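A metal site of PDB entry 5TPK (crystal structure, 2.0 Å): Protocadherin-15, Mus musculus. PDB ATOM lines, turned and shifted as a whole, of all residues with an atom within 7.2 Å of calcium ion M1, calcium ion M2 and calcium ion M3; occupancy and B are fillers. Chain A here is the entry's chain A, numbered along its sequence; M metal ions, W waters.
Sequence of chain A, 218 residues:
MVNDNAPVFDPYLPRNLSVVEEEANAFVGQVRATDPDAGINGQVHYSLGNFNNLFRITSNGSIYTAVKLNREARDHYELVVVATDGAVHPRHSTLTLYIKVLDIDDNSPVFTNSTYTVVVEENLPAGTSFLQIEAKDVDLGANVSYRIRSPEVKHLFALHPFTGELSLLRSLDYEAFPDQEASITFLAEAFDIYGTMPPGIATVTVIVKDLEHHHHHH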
ATOM      1  N   GLU A  21      -6.136 -19.337   2.468  1.00  0.00           N
ATOM      2  CA  GLU A  21      -5.191 -20.331   1.999  1.00  0.00           C
ATOM      3  C   GLU A  21      -4.046 -19.697   1.157  1.00  0.00           C
ATOM      4  O   GLU A  21      -4.152 -18.562   0.682  1.00  0.00           O
ATOM      5  CB  GLU A  21      -5.879 -21.407   1.160  1.00  0.00           C
ATOM      6  CG  GLU A  21      -6.481 -20.936  -0.152  1.00  0.00           C
ATOM      7  CD  GLU A  21      -6.884 -22.065  -1.071  1.00  0.00           C
ATOM      8  OE1 GLU A  21      -7.840 -21.853  -1.855  1.00  0.00           O
ATOM      9  OE2 GLU A  21      -6.252 -23.144  -1.055  1.00  0.00           O
ATOM     10  N   GLU A  22      -2.987 -20.492   0.973  1.00  0.00           N
ATOM     11  CA  GLU A  22      -1.895 -20.214   0.041  1.00  0.00           C
ATOM     12  C   GLU A  22      -1.064 -18.967   0.403  1.00  0.00           C
ATOM     13  O   GLU A  22      -0.600 -18.260  -0.479  1.00  0.00           O
ATOM     14  CB  GLU A  22      -2.390 -20.159  -1.409  1.00  0.00           C
ATOM     15  CG  GLU A  22      -3.195 -21.392  -1.871  1.00  0.00           C
ATOM     16  CD  GLU A  22      -2.400 -22.707  -1.887  1.00  0.00           C
ATOM     17  OE1 GLU A  22      -1.184 -22.736  -1.612  1.00  0.00           O
ATOM     18  OE2 GLU A  22      -3.019 -23.754  -2.187  1.00  0.00           O
ATOM     19  N   LEU A  69      -1.114 -22.761   3.585  1.00  0.00           N
ATOM     20  CA  LEU A  69      -2.162 -23.778   3.802  1.00  0.00           C
ATOM     21  C   LEU A  69      -2.884 -24.001   2.476  1.00  0.00           C
ATOM     22  O   LEU A  69      -3.036 -23.086   1.684  1.00  0.00           O
ATOM     23  CB  LEU A  69      -3.146 -23.356   4.885  1.00  0.00           C
ATOM     24  CG  LEU A  69      -2.508 -23.002   6.242  1.00  0.00           C
ATOM     25  CD1 LEU A  69      -3.565 -22.538   7.221  1.00  0.00           C
ATOM     26  CD2 LEU A  69      -1.727 -24.180   6.824  1.00  0.00           C
ATOM     27  N   ASN A  70      -3.327 -25.233   2.241  1.00  0.00           N
ATOM     28  CA  ASN A  70      -4.065 -25.556   1.035  1.00  0.00           C
ATOM     29  C   ASN A  70      -5.464 -25.996   1.447  1.00  0.00           C
ATOM     30  O   ASN A  70      -5.662 -27.102   1.959  1.00  0.00           O
ATOM     31  CB  ASN A  70      -3.339 -26.660   0.251  1.00  0.00           C
ATOM     32  CG  ASN A  70      -4.030 -27.005  -1.058  1.00  0.00           C
ATOM     33  OD1 ASN A  70      -4.920 -26.286  -1.525  1.00  0.00           O
ATOM     34  ND2 ASN A  70      -3.615 -28.099  -1.663  1.00  0.00           N
ATOM     35  N   ARG A  71      -6.437 -25.124   1.196  1.00  0.00           N
ATOM     36  CA  ARG A  71      -7.837 -25.432   1.528  1.00  0.00           C
ATOM     37  C   ARG A  71      -8.321 -26.723   0.874  1.00  0.00           C
ATOM     38  O   ARG A  71      -9.110 -27.473   1.461  1.00  0.00           O
ATOM     39  CB  ARG A  71      -8.763 -24.288   1.167  1.00  0.00           C
ATOM     40  CG  ARG A  71     -10.106 -24.401   1.871  1.00  0.00           C
ATOM     41  CD  ARG A  71     -11.265 -23.991   1.001  1.00  0.00           C
ATOM     42  NE  ARG A  71     -11.293 -24.617  -0.343  1.00  0.00           N
ATOM     43  CZ  ARG A  71     -11.911 -25.740  -0.706  1.00  0.00           C
ATOM     44  NH1 ARG A  71     -11.852 -26.149  -1.985  1.00  0.00           N
ATOM     45  NH2 ARG A  71     -12.598 -26.456   0.168  1.00  0.00           N
ATOM     46  N   GLU A  72      -7.863 -26.974  -0.348  1.00  0.00           N
ATOM     47  CA  GLU A  72      -8.246 -28.163  -1.102  1.00  0.00           C
ATOM     48  C   GLU A  72      -7.742 -29.445  -0.413  1.00  0.00           C
ATOM     49  O   GLU A  72      -8.295 -30.504  -0.638  1.00  0.00           O
ATOM     50  CB  GLU A  72      -7.757 -28.085  -2.561  1.00  0.00           C
ATOM     51  CG  GLU A  72      -8.637 -27.254  -3.499  1.00  0.00           C
ATOM     52  CD  GLU A  72      -8.577 -25.751  -3.259  1.00  0.00           C
ATOM     53  OE1 GLU A  72      -7.481 -25.165  -3.225  1.00  0.00           O
ATOM     54  OE2 GLU A  72      -9.652 -25.108  -3.163  1.00  0.00           O
ATOM     55  N   ALA A  73      -6.693 -29.337   0.419  1.00  0.00           N
ATOM     56  CA  ALA A  73      -6.169 -30.481   1.169  1.00  0.00           C
ATOM     57  C   ALA A  73      -6.778 -30.571   2.565  1.00  0.00           C
ATOM     58  O   ALA A  73      -7.124 -31.660   3.009  1.00  0.00           O
ATOM     59  CB  ALA A  73      -4.647 -30.413   1.256  1.00  0.00           C
ATOM     60  N   LEU A 102      -9.747 -20.261   4.497  1.00  0.00           N
ATOM     61  CA  LEU A 102     -10.641 -19.672   3.520  1.00  0.00           C
ATOM     62  C   LEU A 102     -10.169 -19.944   2.098  1.00  0.00           C
ATOM     63  O   LEU A 102      -8.975 -19.982   1.852  1.00  0.00           O
ATOM     64  CB  LEU A 102     -10.719 -18.164   3.753  1.00  0.00           C
ATOM     65  CG  LEU A 102     -11.357 -17.770   5.079  1.00  0.00           C
ATOM     66  CD1 LEU A 102     -11.101 -16.296   5.347  1.00  0.00           C
ATOM     67  CD2 LEU A 102     -12.847 -18.095   5.054  1.00  0.00           C
ATOM     68  N   ASP A 103     -11.125 -20.111   1.195  1.00  0.00           N
ATOM     69  CA  ASP A 103     -10.854 -20.478  -0.198  1.00  0.00           C
ATOM     70  C   ASP A 103     -10.480 -19.278  -1.034  1.00  0.00           C
ATOM     71  O   ASP A 103     -11.077 -18.215  -0.861  1.00  0.00           O
ATOM     72  CB  ASP A 103     -12.108 -21.077  -0.846  1.00  0.00           C
ATOM     73  CG  ASP A 103     -11.816 -21.807  -2.152  1.00  0.00           C
ATOM     74  OD1 ASP A 103     -10.906 -22.658  -2.161  1.00  0.00           O
ATOM     75  OD2 ASP A 103     -12.517 -21.564  -3.140  1.00  0.00           O
ATOM     76  N   ILE A 104      -9.528 -19.459  -1.949  1.00  0.00           N
ATOM     77  CA  ILE A 104      -9.321 -18.570  -3.091  1.00  0.00           C
ATOM     78  C   ILE A 104      -9.453 -19.387  -4.358  1.00  0.00           C
ATOM     79  O   ILE A 104      -9.270 -20.598  -4.356  1.00  0.00           O
ATOM     80  CB  ILE A 104      -7.935 -17.857  -3.089  1.00  0.00           C
ATOM     81  CG1 ILE A 104      -6.786 -18.857  -3.376  1.00  0.00           C
ATOM     82  CG2 ILE A 104      -7.711 -17.166  -1.753  1.00  0.00           C
ATOM     83  CD1 ILE A 104      -5.412 -18.225  -3.493  1.00  0.00           C
ATOM     84  N   ASP A 105      -9.754 -18.710  -5.467  1.00  0.00           N
ATOM     85  CA  ASP A 105      -9.722 -19.344  -6.772  1.00  0.00           C
ATOM     86  C   ASP A 105      -8.283 -19.517  -7.241  1.00  0.00           C
ATOM     87  O   ASP A 105      -7.707 -18.627  -7.835  1.00  0.00           O
ATOM     88  CB  ASP A 105     -10.512 -18.534  -7.804  1.00  0.00           C
ATOM     89  CG  ASP A 105     -10.586 -19.221  -9.158  1.00  0.00           C
ATOM     90  OD1 ASP A 105     -10.219 -20.418  -9.260  1.00  0.00           O
ATOM     91  OD2 ASP A 105     -11.010 -18.565 -10.124  1.00  0.00           O
ATOM     92  N   ASP A 106      -7.710 -20.679  -6.945  1.00  0.00           N
ATOM     93  CA  ASP A 106      -6.331 -21.003  -7.359  1.00  0.00           C
ATOM     94  C   ASP A 106      -6.269 -22.272  -8.205  1.00  0.00           C
ATOM     95  O   ASP A 106      -5.185 -22.781  -8.434  1.00  0.00           O
ATOM     96  CB  ASP A 106      -5.389 -21.083  -6.144  1.00  0.00           C
ATOM     97  CG  ASP A 106      -5.802 -22.146  -5.122  1.00  0.00           C
ATOM     98  OD1 ASP A 106      -6.999 -22.507  -5.028  1.00  0.00           O
ATOM     99  OD2 ASP A 106      -4.916 -22.627  -4.379  1.00  0.00           O
ATOM    100  N   ASN A 107      -7.423 -22.766  -8.669  1.00  0.00           N
ATOM    101  CA  ASN A 107      -7.458 -23.888  -9.602  1.00  0.00           C
ATOM    102  C   ASN A 107      -8.363 -23.573 -10.794  1.00  0.00           C
ATOM    103  O   ASN A 107      -9.516 -23.180 -10.618  1.00  0.00           O
ATOM    104  CB  ASN A 107      -7.966 -25.154  -8.939  1.00  0.00           C
ATOM    105  CG  ASN A 107      -7.115 -25.582  -7.782  1.00  0.00           C
ATOM    106  OD1 ASN A 107      -6.186 -26.389  -7.941  1.00  0.00           O
ATOM    107  ND2 ASN A 107      -7.410 -25.050  -6.598  1.00  0.00           N
ATOM    108  N   SER A 108      -7.824 -23.739 -11.978  1.00  0.00           N
ATOM    109  CA  SER A 108      -8.626 -23.734 -13.199  1.00  0.00           C
ATOM    110  C   SER A 108      -9.396 -25.034 -13.315  1.00  0.00           C
ATOM    111  O   SER A 108      -8.924 -26.062 -12.819  1.00  0.00           O
ATOM    112  CB  SER A 108      -7.734 -23.600 -14.425  1.00  0.00           C
ATOM    113  OG  SER A 108      -7.116 -22.349 -14.427  1.00  0.00           O
ATOM    114  N   PRO A 109     -10.566 -25.004 -13.968  1.00  0.00           N
ATOM    115  CA  PRO A 109     -11.206 -26.269 -14.289  1.00  0.00           C
ATOM    116  C   PRO A 109     -10.241 -27.192 -15.039  1.00  0.00           C
ATOM    117  O   PRO A 109      -9.450 -26.700 -15.816  1.00  0.00           O
ATOM    118  CB  PRO A 109     -12.408 -25.860 -15.169  1.00  0.00           C
ATOM    119  CG  PRO A 109     -12.698 -24.471 -14.769  1.00  0.00           C
ATOM    120  CD  PRO A 109     -11.392 -23.852 -14.394  1.00  0.00           C
ATOM    121  N   LYS A 136     -13.695 -30.376 -14.134  1.00  0.00           N
ATOM    122  CA  LYS A 136     -13.992 -30.211 -12.700  1.00  0.00           C
ATOM    123  C   LYS A 136     -13.139 -29.089 -12.138  1.00  0.00           C
ATOM    124  O   LYS A 136     -11.962 -28.971 -12.474  1.00  0.00           O
ATOM    125  CB  LYS A 136     -13.726 -31.513 -11.972  1.00  0.00           C
ATOM    126  CG  LYS A 136     -14.774 -32.573 -12.278  1.00  0.00           C
ATOM    127  CD  LYS A 136     -14.320 -33.976 -11.848  1.00  0.00           C
ATOM    128  CE  LYS A 136     -14.912 -35.050 -12.757  1.00  0.00           C
ATOM    129  NZ  LYS A 136     -14.264 -36.366 -12.493  1.00  0.00           N
ATOM    130  N   ASP A 137     -13.752 -28.250 -11.315  1.00  0.00           N
ATOM    131  CA  ASP A 137     -13.055 -27.206 -10.600  1.00  0.00           C
ATOM    132  C   ASP A 137     -13.074 -27.507  -9.109  1.00  0.00           C
ATOM    133  O   ASP A 137     -14.122 -27.480  -8.477  1.00  0.00           O
ATOM    134  CB  ASP A 137     -13.738 -25.871 -10.887  1.00  0.00           C
ATOM    135  CG  ASP A 137     -12.904 -24.685 -10.475  1.00  0.00           C
ATOM    136  OD1 ASP A 137     -12.304 -24.703  -9.359  1.00  0.00           O
ATOM    137  OD2 ASP A 137     -12.833 -23.705 -11.250  1.00  0.00           O
ATOM    138  N   VAL A 138     -11.892 -27.761  -8.546  1.00  0.00           N
ATOM    139  CA  VAL A 138     -11.757 -28.145  -7.127  1.00  0.00           C
ATOM    140  C   VAL A 138     -12.014 -27.019  -6.102  1.00  0.00           C
ATOM    141  O   VAL A 138     -12.134 -27.284  -4.906  1.00  0.00           O
ATOM    142  CB  VAL A 138     -10.401 -28.834  -6.829  1.00  0.00           C
ATOM    143  CG1 VAL A 138     -10.251 -30.101  -7.678  1.00  0.00           C
ATOM    144  CG2 VAL A 138      -9.216 -27.909  -7.048  1.00  0.00           C
ATOM    145  N   ASP A 139     -12.092 -25.770  -6.556  1.00  0.00           N
ATOM    146  CA  ASP A 139     -12.344 -24.636  -5.643  1.00  0.00           C
ATOM    147  C   ASP A 139     -13.785 -24.620  -5.175  1.00  0.00           C
ATOM    148  O   ASP A 139     -14.659 -25.233  -5.769  1.00  0.00           O
ATOM    149  CB  ASP A 139     -12.002 -23.307  -6.294  1.00  0.00           C
ATOM    150  CG  ASP A 139     -10.525 -23.190  -6.635  1.00  0.00           C
ATOM    151  OD1 ASP A 139      -9.669 -23.418  -5.742  1.00  0.00           O
ATOM    152  OD2 ASP A 139     -10.212 -22.888  -7.803  1.00  0.00           O
ATOM    153  N   LEU A 140     -14.004 -23.885  -4.090  1.00  0.00           N
ATOM    154  CA  LEU A 140     -15.292 -23.847  -3.396  1.00  0.00           C
ATOM    155  C   LEU A 140     -16.340 -23.038  -4.179  1.00  0.00           C
ATOM    156  O   LEU A 140     -16.087 -21.923  -4.589  1.00  0.00           O
ATOM    157  CB  LEU A 140     -15.079 -23.230  -1.998  1.00  0.00           C
ATOM    158  CG  LEU A 140     -16.065 -23.523  -0.879  1.00  0.00           C
ATOM    159  CD1 LEU A 140     -16.141 -25.015  -0.616  1.00  0.00           C
ATOM    160  CD2 LEU A 140     -15.618 -22.792   0.372  1.00  0.00           C
ATOM    161  N   ALA A 142     -17.526 -23.368  -7.177  1.00  0.00           N
ATOM    162  CA  ALA A 142     -17.234 -23.112  -8.573  1.00  0.00           C
ATOM    163  C   ALA A 142     -18.391 -23.677  -9.407  1.00  0.00           C
ATOM    164  O   ALA A 142     -18.977 -24.688  -9.041  1.00  0.00           O
ATOM    165  CB  ALA A 142     -15.924 -23.752  -8.952  1.00  0.00           C
ATOM    166  N   ASP A 192     -14.840 -21.126 -14.696  1.00  0.00           N
ATOM    167  CA  ASP A 192     -15.664 -20.766 -13.545  1.00  0.00           C
ATOM    168  C   ASP A 192     -16.283 -19.414 -13.864  1.00  0.00           C
ATOM    169  O   ASP A 192     -15.585 -18.413 -14.037  1.00  0.00           O
ATOM    170  CB  ASP A 192     -14.862 -20.705 -12.228  1.00  0.00           C
ATOM    171  CG  ASP A 192     -15.757 -20.585 -10.979  1.00  0.00           C
ATOM    172  OD1 ASP A 192     -16.993 -20.420 -11.107  1.00  0.00           O
ATOM    173  OD2 ASP A 192     -15.206 -20.649  -9.846  1.00  0.00           O
ATOM    174  N   GLY A 195     -15.198 -17.082 -11.295  1.00  0.00           N
ATOM    175  CA  GLY A 195     -13.797 -17.240 -10.917  1.00  0.00           C
ATOM    176  C   GLY A 195     -12.888 -16.278 -11.660  1.00  0.00           C
ATOM    177  O   GLY A 195     -13.334 -15.551 -12.552  1.00  0.00           O
ATOM    178  N   THR A 196     -11.613 -16.278 -11.274  1.00  0.00           N
ATOM    179  CA  THR A 196     -10.588 -15.423 -11.846  1.00  0.00           C
ATOM    180  C   THR A 196      -9.422 -16.165 -12.499  1.00  0.00           C
ATOM    181  O   THR A 196      -8.594 -15.527 -13.167  1.00  0.00           O
ATOM    182  CB  THR A 196      -9.986 -14.529 -10.752  1.00  0.00           C
ATOM    183  OG1 THR A 196      -9.462 -15.343  -9.689  1.00  0.00           O
ATOM    184  CG2 THR A 196     -11.037 -13.572 -10.196  1.00  0.00           C
ATOM    185  N   MET A 197      -9.319 -17.473 -12.291  1.00  0.00           N
ATOM    186  CA  MET A 197      -8.247 -18.260 -12.901  1.00  0.00           C
ATOM    187  C   MET A 197      -8.519 -18.385 -14.402  1.00  0.00           C
ATOM    188  O   MET A 197      -9.646 -18.149 -14.851  1.00  0.00           O
ATOM    189  CB  MET A 197      -8.157 -19.660 -12.263  1.00  0.00           C
ATOM    190  CG  MET A 197      -7.402 -19.686 -10.943  1.00  0.00           C
ATOM    191  SD  MET A 197      -5.616 -19.574 -11.144  1.00  0.00           S
ATOM    192  CE  MET A 197      -5.169 -21.260 -11.555  1.00  0.00           C
ATOM    193  N   PRO A 198      -7.486 -18.767 -15.187  1.00  0.00           N
ATOM    194  CA  PRO A 198      -7.723 -19.018 -16.612  1.00  0.00           C
ATOM    195  C   PRO A 198      -8.698 -20.181 -16.838  1.00  0.00           C
ATOM    196  O   PRO A 198      -8.891 -20.998 -15.933  1.00  0.00           O
ATOM    197  CB  PRO A 198      -6.330 -19.371 -17.160  1.00  0.00           C
ATOM    198  CG  PRO A 198      -5.367 -18.876 -16.142  1.00  0.00           C
ATOM    199  CD  PRO A 198      -6.071 -18.956 -14.825  1.00  0.00           C
HETATM  200 CA    CA M   1     -11.406 -22.352  -9.762  1.00  0.00          CA
HETATM  201 CA    CA M   2      -8.940 -22.821  -3.648  1.00  0.00          CA
HETATM  202 CA    CA M   3      -5.311 -24.412  -2.819  1.00  0.00          CA
HETATM  203  O   HOH W   1     -11.732 -20.846 -11.645  1.00  0.00           O
HETATM  204  O   HOH W   2     -12.984 -21.303  -8.905  1.00  0.00           O
HETATM  205  O   HOH W   3      -4.750 -25.676  -4.722  1.00  0.00           O
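Along chain A the residues within 4 Å of calcium ion M2 span positions 21 to 139.
The nearest printed residue that does not touch calcium ion M2 is Asn 107 (4.001 Å).
The side-chain carboxylate (OD1) of Asp 106 sits close to the side-chain amide nitrogen (ND2) of Asn 107 (3.0 Å).
OE2 of Glu 21 sits close to N of Arg 71 (3.0 Å).
The backbone carbonyl oxygen (O) of Leu 102 lies within hydrogen-bond range of the backbone NH (N) of Glu 21, at 3.0 Å.
N of Met 197 is in hydrogen-bond range of OD2 of Asp 105.
OD2 of Asp 105 sits at hydrogen-bond distance from N of Thr 196 (2.6 Å).
N of Glu 22 lies within hydrogen-bond range of O of Leu 69, 2.7 Å away.
The side-chain carboxylate of Asp 103 lies close to the guanidinium group of Arg 71.
The backbone NH (N) of Leu 140 lies within hydrogen-bond range of the side-chain carboxylate (OD2) of Asp 103 (2.9 Å).
Five residues have an atom within 4 Å of calcium ion M3: Glu 21, Glu 22, Asn 70, Glu 72 and Asp 106.
Calcium ion M2 is bound by OD1 of Asp 139 (2.3 Å), OE1 of Glu 21 (2.3 Å), O of Ile 104 (2.4 Å), OD1 of Asp 106 (2.4 Å), OE2 of Glu 72 (2.4 Å), OD1 of Asp 103 (2.5 Å) and OE1 of Glu 72 (2.8 Å).
Calcium ion M2 has seven donor atoms within binding distance.
Water W2 is bound to calcium ion M1 (2.1 Å).
Calcium ion M1 is bound by O of Asn 107 (2.2 Å).
The side-chain carboxylate (OD1) of Asp 105 binds calcium ion M1.
OD2 of Asp 139 binds calcium ion M1.
Water W1 is bound to calcium ion M1 (2.4 Å).
OD2 of Asp 137 is bound to calcium ion M1, at 2.5 Å.
Calcium ion M1 is bound by the side-chain carboxylate (OD1) of Asp 137 (2.5 Å).
Calcium ion M1 has seven donor atoms within binding distance.
Four residues have an atom within 4 Å of calcium ion M1: Asp 105, Asn 107, Asp 137 and Asp 139.
Along chain A the residues within 4 Å of calcium ion M1 span positions 105 to 139.
The nearest printed residue that does not touch calcium ion M1 is Asp 192 (4.2 Å).
Calcium ion M3 is bound by OD1 of Asn 70 (2.3 Å), OE1 of Glu 72 (2.3 Å), water W3 (2.4 Å), OE2 of Glu 21 (2.4 Å), OD2 of Asp 106 (2.4 Å) and OE2 of Glu 22 (2.5 Å).
Calcium ion M3 has six donor atoms within binding distance.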
